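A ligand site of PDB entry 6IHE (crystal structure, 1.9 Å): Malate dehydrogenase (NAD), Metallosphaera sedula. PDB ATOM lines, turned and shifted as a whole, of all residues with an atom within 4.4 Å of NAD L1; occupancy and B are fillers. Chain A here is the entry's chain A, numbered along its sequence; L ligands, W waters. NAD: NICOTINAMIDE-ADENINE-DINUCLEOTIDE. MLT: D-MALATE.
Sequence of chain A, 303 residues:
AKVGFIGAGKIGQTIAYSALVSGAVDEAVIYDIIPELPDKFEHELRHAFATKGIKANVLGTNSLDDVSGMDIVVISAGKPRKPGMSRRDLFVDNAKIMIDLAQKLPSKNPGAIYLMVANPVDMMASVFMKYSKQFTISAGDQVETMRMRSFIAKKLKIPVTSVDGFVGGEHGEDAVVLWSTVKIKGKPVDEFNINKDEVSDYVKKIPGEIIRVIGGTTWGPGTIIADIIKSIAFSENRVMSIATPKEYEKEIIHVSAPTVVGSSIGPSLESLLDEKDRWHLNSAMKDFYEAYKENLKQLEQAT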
ATOM      1  N   ALA A   8     -17.882  10.198  -0.396  1.00  0.00           N
ATOM      2  CA  ALA A   8     -17.514   9.009  -1.167  1.00  0.00           C
ATOM      3  C   ALA A   8     -17.247   9.330  -2.599  1.00  0.00           C
ATOM      4  O   ALA A   8     -17.574   8.539  -3.518  1.00  0.00           O
ATOM      5  CB  ALA A   8     -18.554   7.904  -1.068  1.00  0.00           C
ATOM      6  N   GLY A   9     -16.557  10.434  -2.795  1.00  0.00           N
ATOM      7  CA  GLY A   9     -15.955  10.755  -4.074  1.00  0.00           C
ATOM      8  C   GLY A   9     -14.627   9.961  -4.265  1.00  0.00           C
ATOM      9  O   GLY A   9     -14.405   8.933  -3.617  1.00  0.00           O
ATOM     10  N   LYS A  10     -13.775  10.414  -5.188  1.00  0.00           N
ATOM     11  CA  LYS A  10     -12.478   9.750  -5.464  1.00  0.00           C
ATOM     12  C   LYS A  10     -11.619   9.545  -4.232  1.00  0.00           C
ATOM     13  O   LYS A  10     -11.260   8.444  -3.937  1.00  0.00           O
ATOM     14  CB  LYS A  10     -11.699  10.509  -6.518  1.00  0.00           C
ATOM     15  CG  LYS A  10     -12.297  10.336  -7.903  1.00  0.00           C
ATOM     16  CD  LYS A  10     -11.305  10.784  -8.995  1.00  0.00           C
ATOM     17  CE  LYS A  10     -10.809  12.227  -8.818  1.00  0.00           C
ATOM     18  NZ  LYS A  10     -11.937  13.197  -8.772  1.00  0.00           N
ATOM     19  N   ILE A  11     -11.360  10.572  -3.445  1.00  0.00           N
ATOM     20  CA  ILE A  11     -10.490  10.386  -2.341  1.00  0.00           C
ATOM     21  C   ILE A  11     -11.157   9.618  -1.204  1.00  0.00           C
ATOM     22  O   ILE A  11     -10.511   8.850  -0.565  1.00  0.00           O
ATOM     23  CB  ILE A  11      -9.883  11.724  -1.849  1.00  0.00           C
ATOM     24  CG1 ILE A  11      -8.645  11.497  -0.995  1.00  0.00           C
ATOM     25  CG2 ILE A  11     -10.893  12.499  -1.044  1.00  0.00           C
ATOM     26  CD1 ILE A  11      -7.557  10.702  -1.709  1.00  0.00           C
ATOM     27  N   GLY A  12     -12.448   9.850  -0.930  1.00  0.00           N
ATOM     28  CA  GLY A  12     -13.144   9.112   0.121  1.00  0.00           C
ATOM     29  C   GLY A  12     -13.186   7.625  -0.188  1.00  0.00           C
ATOM     30  O   GLY A  12     -12.949   6.846   0.639  1.00  0.00           O
ATOM     31  N   TYR A  31     -21.088   7.659   3.878  1.00  0.00           N
ATOM     32  CA  TYR A  31     -22.103   8.573   3.441  1.00  0.00           C
ATOM     33  C   TYR A  31     -21.673   9.512   2.311  1.00  0.00           C
ATOM     34  O   TYR A  31     -20.561   9.894   2.243  1.00  0.00           O
ATOM     35  CB  TYR A  31     -22.603   9.416   4.648  1.00  0.00           C
ATOM     36  CG  TYR A  31     -23.335  10.676   4.281  1.00  0.00           C
ATOM     37  CD1 TYR A  31     -24.636  10.622   3.859  1.00  0.00           C
ATOM     38  CD2 TYR A  31     -22.697  11.883   4.288  1.00  0.00           C
ATOM     39  CE1 TYR A  31     -25.300  11.756   3.477  1.00  0.00           C
ATOM     40  CE2 TYR A  31     -23.353  13.028   3.925  1.00  0.00           C
ATOM     41  CZ  TYR A  31     -24.665  12.961   3.514  1.00  0.00           C
ATOM     42  OH  TYR A  31     -25.319  14.064   3.108  1.00  0.00           O
ATOM     43  N   ASP A  32     -22.606   9.907   1.461  1.00  0.00           N
ATOM     44  CA  ASP A  32     -22.395  10.885   0.422  1.00  0.00           C
ATOM     45  C   ASP A  32     -23.738  11.542   0.093  1.00  0.00           C
ATOM     46  O   ASP A  32     -24.737  10.915   0.165  1.00  0.00           O
ATOM     47  CB  ASP A  32     -21.734  10.343  -0.831  1.00  0.00           C
ATOM     48  CG  ASP A  32     -21.046  11.423  -1.642  1.00  0.00           C
ATOM     49  OD1 ASP A  32     -21.696  12.060  -2.447  1.00  0.00           O
ATOM     50  OD2 ASP A  32     -19.876  11.667  -1.463  1.00  0.00           O
ATOM     51  N   ILE A  33     -23.716  12.807  -0.287  1.00  0.00           N
ATOM     52  CA  ILE A  33     -24.893  13.531  -0.645  1.00  0.00           C
ATOM     53  C   ILE A  33     -25.387  13.137  -2.008  1.00  0.00           C
ATOM     54  O   ILE A  33     -26.493  13.329  -2.324  1.00  0.00           O
ATOM     55  CB  ILE A  33     -24.701  15.040  -0.573  1.00  0.00           C
ATOM     56  CG1 ILE A  33     -26.029  15.737  -0.524  1.00  0.00           C
ATOM     57  CG2 ILE A  33     -23.892  15.547  -1.729  1.00  0.00           C
ATOM     58  CD1 ILE A  33     -25.946  17.061   0.165  1.00  0.00           C
ATOM     59  N   ILE A  34     -24.534  12.563  -2.820  1.00  0.00           N
ATOM     60  CA  ILE A  34     -24.933  12.129  -4.168  1.00  0.00           C
ATOM     61  C   ILE A  34     -25.791  10.910  -4.105  1.00  0.00           C
ATOM     62  O   ILE A  34     -25.444   9.928  -3.425  1.00  0.00           O
ATOM     63  CB  ILE A  34     -23.703  11.903  -5.102  1.00  0.00           C
ATOM     64  CG1 ILE A  34     -23.099  13.257  -5.431  1.00  0.00           C
ATOM     65  CG2 ILE A  34     -24.084  11.192  -6.378  1.00  0.00           C
ATOM     66  CD1 ILE A  34     -21.674  13.164  -5.972  1.00  0.00           C
ATOM     67  N   LEU A  37     -24.645   6.728  -4.785  1.00  0.00           N
ATOM     68  CA  LEU A  37     -23.187   6.626  -4.983  1.00  0.00           C
ATOM     69  C   LEU A  37     -22.630   5.735  -3.854  1.00  0.00           C
ATOM     70  O   LEU A  37     -22.008   4.698  -4.136  1.00  0.00           O
ATOM     71  CB  LEU A  37     -22.493   8.018  -5.039  1.00  0.00           C
ATOM     72  CG  LEU A  37     -20.948   8.056  -4.910  1.00  0.00           C
ATOM     73  CD1 LEU A  37     -20.302   7.199  -5.986  1.00  0.00           C
ATOM     74  CD2 LEU A  37     -20.480   9.489  -5.057  1.00  0.00           C
ATOM     75  N   SER A  76     -14.068  13.946   3.831  1.00  0.00           N
ATOM     76  CA  SER A  76     -13.588  14.328   2.516  1.00  0.00           C
ATOM     77  C   SER A  76     -14.636  15.048   1.640  1.00  0.00           C
ATOM     78  O   SER A  76     -14.348  15.396   0.489  1.00  0.00           O
ATOM     79  CB  SER A  76     -13.012  13.096   1.797  1.00  0.00           C
ATOM     80  OG  SER A  76     -14.016  12.233   1.359  1.00  0.00           O
ATOM     81  N   ALA A  77     -15.834  15.295   2.182  1.00  0.00           N
ATOM     82  CA  ALA A  77     -16.865  16.008   1.440  1.00  0.00           C
ATOM     83  C   ALA A  77     -16.412  17.427   1.138  1.00  0.00           C
ATOM     84  O   ALA A  77     -16.155  18.214   2.073  1.00  0.00           O
ATOM     85  CB  ALA A  77     -18.152  16.072   2.264  1.00  0.00           C
ATOM     86  N   GLY A  78     -16.276  17.735  -0.135  1.00  0.00           N
ATOM     87  CA  GLY A  78     -15.981  19.116  -0.545  1.00  0.00           C
ATOM     88  C   GLY A  78     -15.614  19.248  -2.013  1.00  0.00           C
ATOM     89  O   GLY A  78     -15.360  18.241  -2.699  1.00  0.00           O
ATOM     90  N   LYS A  79     -15.620  20.489  -2.482  1.00  0.00           N
ATOM     91  CA  LYS A  79     -15.184  20.789  -3.859  1.00  0.00           C
ATOM     92  C   LYS A  79     -13.640  20.521  -3.922  1.00  0.00           C
ATOM     93  O   LYS A  79     -12.911  20.969  -3.015  1.00  0.00           O
ATOM     94  CB  LYS A  79     -15.452  22.246  -4.228  1.00  0.00           C
ATOM     95  CG  LYS A  79     -16.895  22.747  -4.079  1.00  0.00           C
ATOM     96  CD  LYS A  79     -17.724  22.640  -5.372  1.00  0.00           C
ATOM     97  CE  LYS A  79     -19.064  23.371  -5.315  1.00  0.00           C
ATOM     98  NZ  LYS A  79     -20.150  22.499  -4.777  1.00  0.00           N
ATOM     99  N   PRO A  80     -13.160  19.872  -4.955  1.00  0.00           N
ATOM    100  CA  PRO A  80     -11.730  19.655  -5.127  1.00  0.00           C
ATOM    101  C   PRO A  80     -11.205  20.738  -6.045  1.00  0.00           C
ATOM    102  O   PRO A  80     -11.965  21.484  -6.572  1.00  0.00           O
ATOM    103  CB  PRO A  80     -11.663  18.346  -5.865  1.00  0.00           C
ATOM    104  CG  PRO A  80     -12.895  18.323  -6.646  1.00  0.00           C
ATOM    105  CD  PRO A  80     -13.922  18.918  -5.752  1.00  0.00           C
ATOM    106  N   ARG A  81      -9.903  20.772  -6.213  1.00  0.00           N
ATOM    107  CA  ARG A  81      -9.228  21.732  -7.062  1.00  0.00           C
ATOM    108  C   ARG A  81      -9.327  21.439  -8.546  1.00  0.00           C
ATOM    109  O   ARG A  81      -9.421  20.324  -8.964  1.00  0.00           O
ATOM    110  CB  ARG A  81      -7.754  21.727  -6.729  1.00  0.00           C
ATOM    111  CG  ARG A  81      -7.356  22.567  -5.562  1.00  0.00           C
ATOM    112  CD  ARG A  81      -5.981  23.137  -5.770  1.00  0.00           C
ATOM    113  NE  ARG A  81      -4.945  22.126  -5.614  1.00  0.00           N
ATOM    114  CZ  ARG A  81      -3.665  22.344  -5.836  1.00  0.00           C
ATOM    115  NH1 ARG A  81      -3.255  23.509  -6.242  1.00  0.00           N
ATOM    116  NH2 ARG A  81      -2.787  21.386  -5.654  1.00  0.00           N
ATOM    117  N   LEU A  90     -10.800  27.301  -2.214  1.00  0.00           N
ATOM    118  CA  LEU A  90     -11.972  26.531  -1.847  1.00  0.00           C
ATOM    119  C   LEU A  90     -12.566  26.924  -0.476  1.00  0.00           C
ATOM    120  O   LEU A  90     -13.591  26.361  -0.093  1.00  0.00           O
ATOM    121  CB  LEU A  90     -11.592  25.033  -1.821  1.00  0.00           C
ATOM    122  CG  LEU A  90     -11.093  24.471  -3.132  1.00  0.00           C
ATOM    123  CD1 LEU A  90     -10.251  23.225  -2.926  1.00  0.00           C
ATOM    124  CD2 LEU A  90     -12.266  24.224  -4.098  1.00  0.00           C
ATOM    125  N   ASN A  94     -16.240  25.194   0.853  1.00  0.00           N
ATOM    126  CA  ASN A  94     -16.169  24.053   1.727  1.00  0.00           C
ATOM    127  C   ASN A  94     -16.378  24.357   3.187  1.00  0.00           C
ATOM    128  O   ASN A  94     -16.820  23.492   3.941  1.00  0.00           O
ATOM    129  CB  ASN A  94     -14.882  23.316   1.452  1.00  0.00           C
ATOM    130  CG  ASN A  94     -14.899  22.707   0.095  1.00  0.00           C
ATOM    131  OD1 ASN A  94     -15.975  22.554  -0.513  1.00  0.00           O
ATOM    132  ND2 ASN A  94     -13.747  22.335  -0.398  1.00  0.00           N
ATOM    133  N   ILE A  97     -19.998  23.702   4.014  1.00  0.00           N
ATOM    134  CA  ILE A  97     -20.139  22.285   4.271  1.00  0.00           C
ATOM    135  C   ILE A  97     -19.737  21.940   5.715  1.00  0.00           C
ATOM    136  O   ILE A  97     -20.514  21.269   6.476  1.00  0.00           O
ATOM    137  CB  ILE A  97     -19.325  21.429   3.272  1.00  0.00           C
ATOM    138  CG1 ILE A  97     -19.894  21.630   1.861  1.00  0.00           C
ATOM    139  CG2 ILE A  97     -19.358  19.948   3.691  1.00  0.00           C
ATOM    140  CD1 ILE A  97     -19.002  21.219   0.729  1.00  0.00           C
ATOM    141  N   VAL A 117     -10.001  15.836   5.679  1.00  0.00           N
ATOM    142  CA  VAL A 117      -9.343  15.545   4.448  1.00  0.00           C
ATOM    143  C   VAL A 117      -9.653  16.618   3.406  1.00  0.00           C
ATOM    144  O   VAL A 117      -8.776  16.942   2.581  1.00  0.00           O
ATOM    145  CB  VAL A 117      -9.779  14.191   3.912  1.00  0.00           C
ATOM    146  CG1 VAL A 117      -9.254  13.975   2.506  1.00  0.00           C
ATOM    147  CG2 VAL A 117      -9.406  13.118   4.874  1.00  0.00           C
ATOM    148  N   ALA A 118     -10.879  17.135   3.397  1.00  0.00           N
ATOM    149  CA  ALA A 118     -11.304  18.149   2.461  1.00  0.00           C
ATOM    150  C   ALA A 118     -10.491  19.439   2.536  1.00  0.00           C
ATOM    151  O   ALA A 118     -10.187  19.927   3.634  1.00  0.00           O
ATOM    152  CB  ALA A 118     -12.778  18.487   2.668  1.00  0.00           C
ATOM    153  N   ASN A 119     -10.170  20.032   1.399  1.00  0.00           N
ATOM    154  CA  ASN A 119      -9.354  21.259   1.355  1.00  0.00           C
ATOM    155  C   ASN A 119     -10.142  22.587   1.488  1.00  0.00           C
ATOM    156  O   ASN A 119     -11.298  22.627   1.205  1.00  0.00           O
ATOM    157  CB  ASN A 119      -8.531  21.279   0.056  1.00  0.00           C
ATOM    158  CG  ASN A 119      -7.262  20.466   0.142  1.00  0.00           C
ATOM    159  OD1 ASN A 119      -6.497  20.647   1.043  1.00  0.00           O
ATOM    160  ND2 ASN A 119      -7.044  19.588  -0.794  1.00  0.00           N
ATOM    161  N   VAL A 121      -7.388  21.806   3.648  1.00  0.00           N
ATOM    162  CA  VAL A 121      -7.369  20.965   4.815  1.00  0.00           C
ATOM    163  C   VAL A 121      -7.161  21.469   6.227  1.00  0.00           C
ATOM    164  O   VAL A 121      -7.916  21.116   7.071  1.00  0.00           O
ATOM    165  CB  VAL A 121      -6.636  19.641   4.578  1.00  0.00           C
ATOM    166  CG1 VAL A 121      -5.156  19.825   4.731  1.00  0.00           C
ATOM    167  CG2 VAL A 121      -7.165  18.590   5.508  1.00  0.00           C
ATOM    168  N   ALA A 139      -5.254  15.721   7.940  1.00  0.00           N
ATOM    169  CA  ALA A 139      -4.223  14.946   7.315  1.00  0.00           C
ATOM    170  C   ALA A 139      -2.921  15.808   7.212  1.00  0.00           C
ATOM    171  O   ALA A 139      -1.791  15.287   7.194  1.00  0.00           O
ATOM    172  CB  ALA A 139      -4.665  14.514   5.908  1.00  0.00           C
ATOM    173  N   VAL A 143       1.004  13.841   3.742  1.00  0.00           N
ATOM    174  CA  VAL A 143       1.053  13.483   2.314  1.00  0.00           C
ATOM    175  C   VAL A 143       2.361  14.045   1.694  1.00  0.00           C
ATOM    176  O   VAL A 143       3.102  13.330   1.027  1.00  0.00           O
ATOM    177  CB  VAL A 143      -0.165  13.991   1.537  1.00  0.00           C
ATOM    178  CG1 VAL A 143      -0.075  13.619   0.012  1.00  0.00           C
ATOM    179  CG2 VAL A 143      -1.455  13.386   2.129  1.00  0.00           C
ATOM    180  N   THR A 217      -5.875  13.839  -7.233  1.00  0.00           N
ATOM    181  CA  THR A 217      -5.009  12.895  -6.567  1.00  0.00           C
ATOM    182  C   THR A 217      -5.845  11.810  -5.855  1.00  0.00           C
ATOM    183  O   THR A 217      -6.917  12.095  -5.289  1.00  0.00           O
ATOM    184  CB  THR A 217      -4.119  13.604  -5.572  1.00  0.00           C
ATOM    185  OG1 THR A 217      -4.928  14.384  -4.706  1.00  0.00           O
ATOM    186  CG2 THR A 217      -3.113  14.549  -6.323  1.00  0.00           C
ATOM    187  N   PRO A 221      -2.435  10.012  -1.679  1.00  0.00           N
ATOM    188  CA  PRO A 221      -3.015  10.512  -0.410  1.00  0.00           C
ATOM    189  C   PRO A 221      -4.037   9.534   0.218  1.00  0.00           C
ATOM    190  O   PRO A 221      -4.134   9.425   1.427  1.00  0.00           O
ATOM    191  CB  PRO A 221      -3.637  11.830  -0.801  1.00  0.00           C
ATOM    192  CG  PRO A 221      -3.725  11.824  -2.282  1.00  0.00           C
ATOM    193  CD  PRO A 221      -2.754  10.855  -2.821  1.00  0.00           C
ATOM    194  N   ILE A 225      -3.437   8.632   3.992  1.00  0.00           N
ATOM    195  CA  ILE A 225      -4.464   8.946   4.990  1.00  0.00           C
ATOM    196  C   ILE A 225      -5.035   7.706   5.654  1.00  0.00           C
ATOM    197  O   ILE A 225      -5.270   7.651   6.875  1.00  0.00           O
ATOM    198  CB  ILE A 225      -5.562   9.851   4.392  1.00  0.00           C
ATOM    199  CG1 ILE A 225      -4.902  11.183   4.004  1.00  0.00           C
ATOM    200  CG2 ILE A 225      -6.696  10.050   5.426  1.00  0.00           C
ATOM    201  CD1 ILE A 225      -5.668  12.132   3.088  1.00  0.00           C
HETATM  202  PA  NAD L   1     -14.867  14.550  -5.751  1.00  0.00           P
HETATM  203  O1A NAD L   1     -15.657  15.640  -6.484  1.00  0.00           O
HETATM  204  O2A NAD L   1     -14.458  13.231  -6.408  1.00  0.00           O
HETATM  205  O5B NAD L   1     -15.760  14.187  -4.485  1.00  0.00           O
HETATM  206  C5B NAD L   1     -16.274  15.121  -3.533  1.00  0.00           C
HETATM  207  C4B NAD L   1     -17.409  14.356  -2.891  1.00  0.00           C
HETATM  208  O4B NAD L   1     -17.898  15.153  -1.848  1.00  0.00           O
HETATM  209  C3B NAD L   1     -18.525  14.124  -3.910  1.00  0.00           C
HETATM  210  O3B NAD L   1     -18.890  12.725  -4.069  1.00  0.00           O
HETATM  211  C2B NAD L   1     -19.619  15.024  -3.408  1.00  0.00           C
HETATM  212  O2B NAD L   1     -20.928  14.522  -3.471  1.00  0.00           O
HETATM  213  C1B NAD L   1     -19.304  15.072  -1.958  1.00  0.00           C
HETATM  214  N9A NAD L   1     -19.962  16.218  -1.325  1.00  0.00           N
HETATM  215  C8A NAD L   1     -19.944  17.527  -1.679  1.00  0.00           C
HETATM  216  N7A NAD L   1     -20.680  18.216  -0.750  1.00  0.00           N
HETATM  217  C5A NAD L   1     -21.138  17.357   0.192  1.00  0.00           C
HETATM  218  C6A NAD L   1     -21.969  17.433   1.427  1.00  0.00           C
HETATM  219  N6A NAD L   1     -22.422  18.643   1.799  1.00  0.00           N
HETATM  220  N1A NAD L   1     -22.254  16.273   2.124  1.00  0.00           N
HETATM  221  C2A NAD L   1     -21.766  15.058   1.675  1.00  0.00           C
HETATM  222  N3A NAD L   1     -21.018  14.864   0.550  1.00  0.00           N
HETATM  223  C4A NAD L   1     -20.684  16.002  -0.194  1.00  0.00           C
HETATM  224  O3  NAD L   1     -13.613  15.190  -4.950  1.00  0.00           O
HETATM  225  PN  NAD L   1     -12.361  14.352  -4.285  1.00  0.00           P
HETATM  226  O1N NAD L   1     -11.310  14.192  -5.360  1.00  0.00           O
HETATM  227  O2N NAD L   1     -12.834  13.102  -3.607  1.00  0.00           O
HETATM  228  O5D NAD L   1     -11.947  15.506  -3.225  1.00  0.00           O
HETATM  229  C5D NAD L   1     -12.716  15.792  -2.091  1.00  0.00           C
HETATM  230  C4D NAD L   1     -11.987  16.806  -1.243  1.00  0.00           C
HETATM  231  O4D NAD L   1     -10.761  16.243  -0.732  1.00  0.00           O
HETATM  232  C3D NAD L   1     -11.572  18.058  -1.996  1.00  0.00           C
HETATM  233  O3D NAD L   1     -11.620  19.213  -1.123  1.00  0.00           O
HETATM  234  C2D NAD L   1     -10.092  17.812  -2.400  1.00  0.00           C
HETATM  235  O2D NAD L   1      -9.357  19.049  -2.639  1.00  0.00           O
HETATM  236  C1D NAD L   1      -9.630  17.058  -1.145  1.00  0.00           C
HETATM  237  N1N NAD L   1      -8.439  16.167  -1.221  1.00  0.00           N
HETATM  238  C2N NAD L   1      -7.528  16.283  -0.211  1.00  0.00           C
HETATM  239  C3N NAD L   1      -6.390  15.484  -0.115  1.00  0.00           C
HETATM  240  C7N NAD L   1      -5.477  15.688   1.046  1.00  0.00           C
HETATM  241  O7N NAD L   1      -5.830  16.205   2.114  1.00  0.00           O
HETATM  242  N7N NAD L   1      -4.266  15.222   0.937  1.00  0.00           N
HETATM  243  C4N NAD L   1      -6.169  14.569  -1.141  1.00  0.00           C
HETATM  244  C5N NAD L   1      -7.114  14.464  -2.192  1.00  0.00           C
HETATM  245  C6N NAD L   1      -8.240  15.281  -2.221  1.00  0.00           C
HETATM  246  C1  MLT L   2      -2.930  16.732  -2.502  1.00  0.00           C
HETATM  247  O1  MLT L   2      -1.869  17.124  -1.985  1.00  0.00           O
HETATM  248  O2  MLT L   2      -3.052  15.684  -3.194  1.00  0.00           O
HETATM  249  C2  MLT L   2      -3.992  17.794  -2.307  1.00  0.00           C
HETATM  250  O3  MLT L   2      -4.286  18.244  -1.005  1.00  0.00           O
HETATM  251  C3  MLT L   2      -5.233  17.679  -3.180  1.00  0.00           C
HETATM  252  C4  MLT L   2      -5.033  18.945  -4.024  1.00  0.00           C
HETATM  253  O4  MLT L   2      -5.926  19.824  -4.199  1.00  0.00           O
HETATM  254  O5  MLT L   2      -3.876  19.088  -4.484  1.00  0.00           O
HETATM  255  O   HOH W   1      -8.104  18.703  -4.871  1.00  0.00           O
HETATM  256  O   HOH W   2     -22.439  20.096  -0.995  1.00  0.00           O
HETATM  257  O   HOH W   3      -8.646  14.108  -5.715  1.00  0.00           O
HETATM  258  O   HOH W   4      -3.483  16.527   3.560  1.00  0.00           O
HETATM  259  O   HOH W   5      -2.147  17.070   0.812  1.00  0.00           O
HETATM  260  O   HOH W   6     -14.474  12.084  -1.428  1.00  0.00           O
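O2B of NAD L1 lies within hydrogen-bond range of OD1 of Asp 32 (2.8 Å). An oxygen (O3D) of NAD L1 sits at hydrogen-bond distance from the backbone carbonyl oxygen (O) of Lys 79, at 2.9 Å. The backbone NH of Ile 11 lies within hydrogen-bond range of an oxygen (O2N) of NAD L1 (2.9 Å). An oxygen (O3D) of NAD L1 is in hydrogen-bond range of the backbone NH (N) of Asn 119. O2D of NAD L1 lies within hydrogen-bond range of ND2 of Asn 119 (3.0 Å). N of Lys 10 lies within hydrogen-bond range of O2A of NAD L1, at 3.1 Å. The side-chain amino group of Lys 10 lies within salt-bridge range of an oxygen (O2A) of NAD L1 (3.5 Å). N of Gly 78 is in hydrogen-bond range of O4B of NAD L1, 3.5 Å away. A nitrogen (N3A) of NAD L1 is in hydrogen-bond range of the backbone NH (N) of Ile 33. An oxygen (O3) of MLT L2 lies within hydrogen-bond range of the side-chain amide nitrogen (ND2) of Asn 119, at 3.1 Å. The side-chain hydroxyl (OG1) of Thr 217 is in hydrogen-bond range of an oxygen (O2) of MLT L2. The guanidinium group of Arg 81 is in salt-bridge range of an oxygen (O5) of MLT L2, 2.8 Å away.
The side-chain carboxylate of Asp 32 sits at hydrogen-bond distance from the backbone NH of Ile 34 (2.9 Å). The side-chain carboxylate (OD2) of Asp 32 is in hydrogen-bond range of the backbone NH (N) of Ala 8 (2.7 Å). The backbone NH of Lys 79 lies within hydrogen-bond range of the side-chain amide oxygen of Asn 94 (2.9 Å). The backbone carbonyl oxygen (O) of Asn 119 is in hydrogen-bond range of the side-chain amide nitrogen (ND2) of Asn 94. The backbone NH of Val 121 sits at hydrogen-bond distance from the side-chain amide oxygen of Asn 119 (3.0 Å).
O7N of NAD L1 sits close to O of Val 117. Residues that only touch NAD L1: Ile 34 (2.9 Å), Ser 76 (3.1 Å), Thr 217 (3.3 Å), Tyr 31 (3.4 Å), Gly 9 (3.5 Å), Pro 80 (3.5 Å), Ala 77 (3.5 Å), Val 143 (3.6 Å), Leu 37 (3.7 Å), Ile 97 (3.7 Å), Pro 221 (3.7 Å), Ala 118 (3.8 Å) and Asn 94 (3.8 Å). 21 residues have an atom within 4 Å of NAD L1: Gly 9, Lys 10, Ile 11, Tyr 31, Asp 32, Ile 33, Ile 34, Leu 37, Ser 76, Ala 77, Gly 78, Lys 79, Pro 80, Asn 94, Ile 97, Val 117, Ala 118, Asn 119, Val 143, Thr 217 and Pro 221. The nearest printed residue that does not touch NAD L1 is Arg 81 (4.01 Å).
Water W1 lies within hydrogen-bond range of an oxygen (O4) of MLT L2 (2.5 Å), an oxygen (O2D) of NAD L1 (2.6 Å) and the backbone NH (N) of Arg 81 (3.1 Å). Water W3 bridges the backbone carbonyl oxygen of Thr 217 (2.7 Å) and an oxygen (O1N) of NAD L1 (2.7 Å). Water W5 lies within hydrogen-bond range of an oxygen (O1) of MLT L2 (2.8 Å) and a nitrogen (N7N) of NAD L1 (2.8 Å). Water W6 lies within hydrogen-bond range of OG of Ser 76 (2.8 Å), O2N of NAD L1 (2.9 Å), N of Gly 9 (3.0 Å) and N of Gly 12 (3.1 Å).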
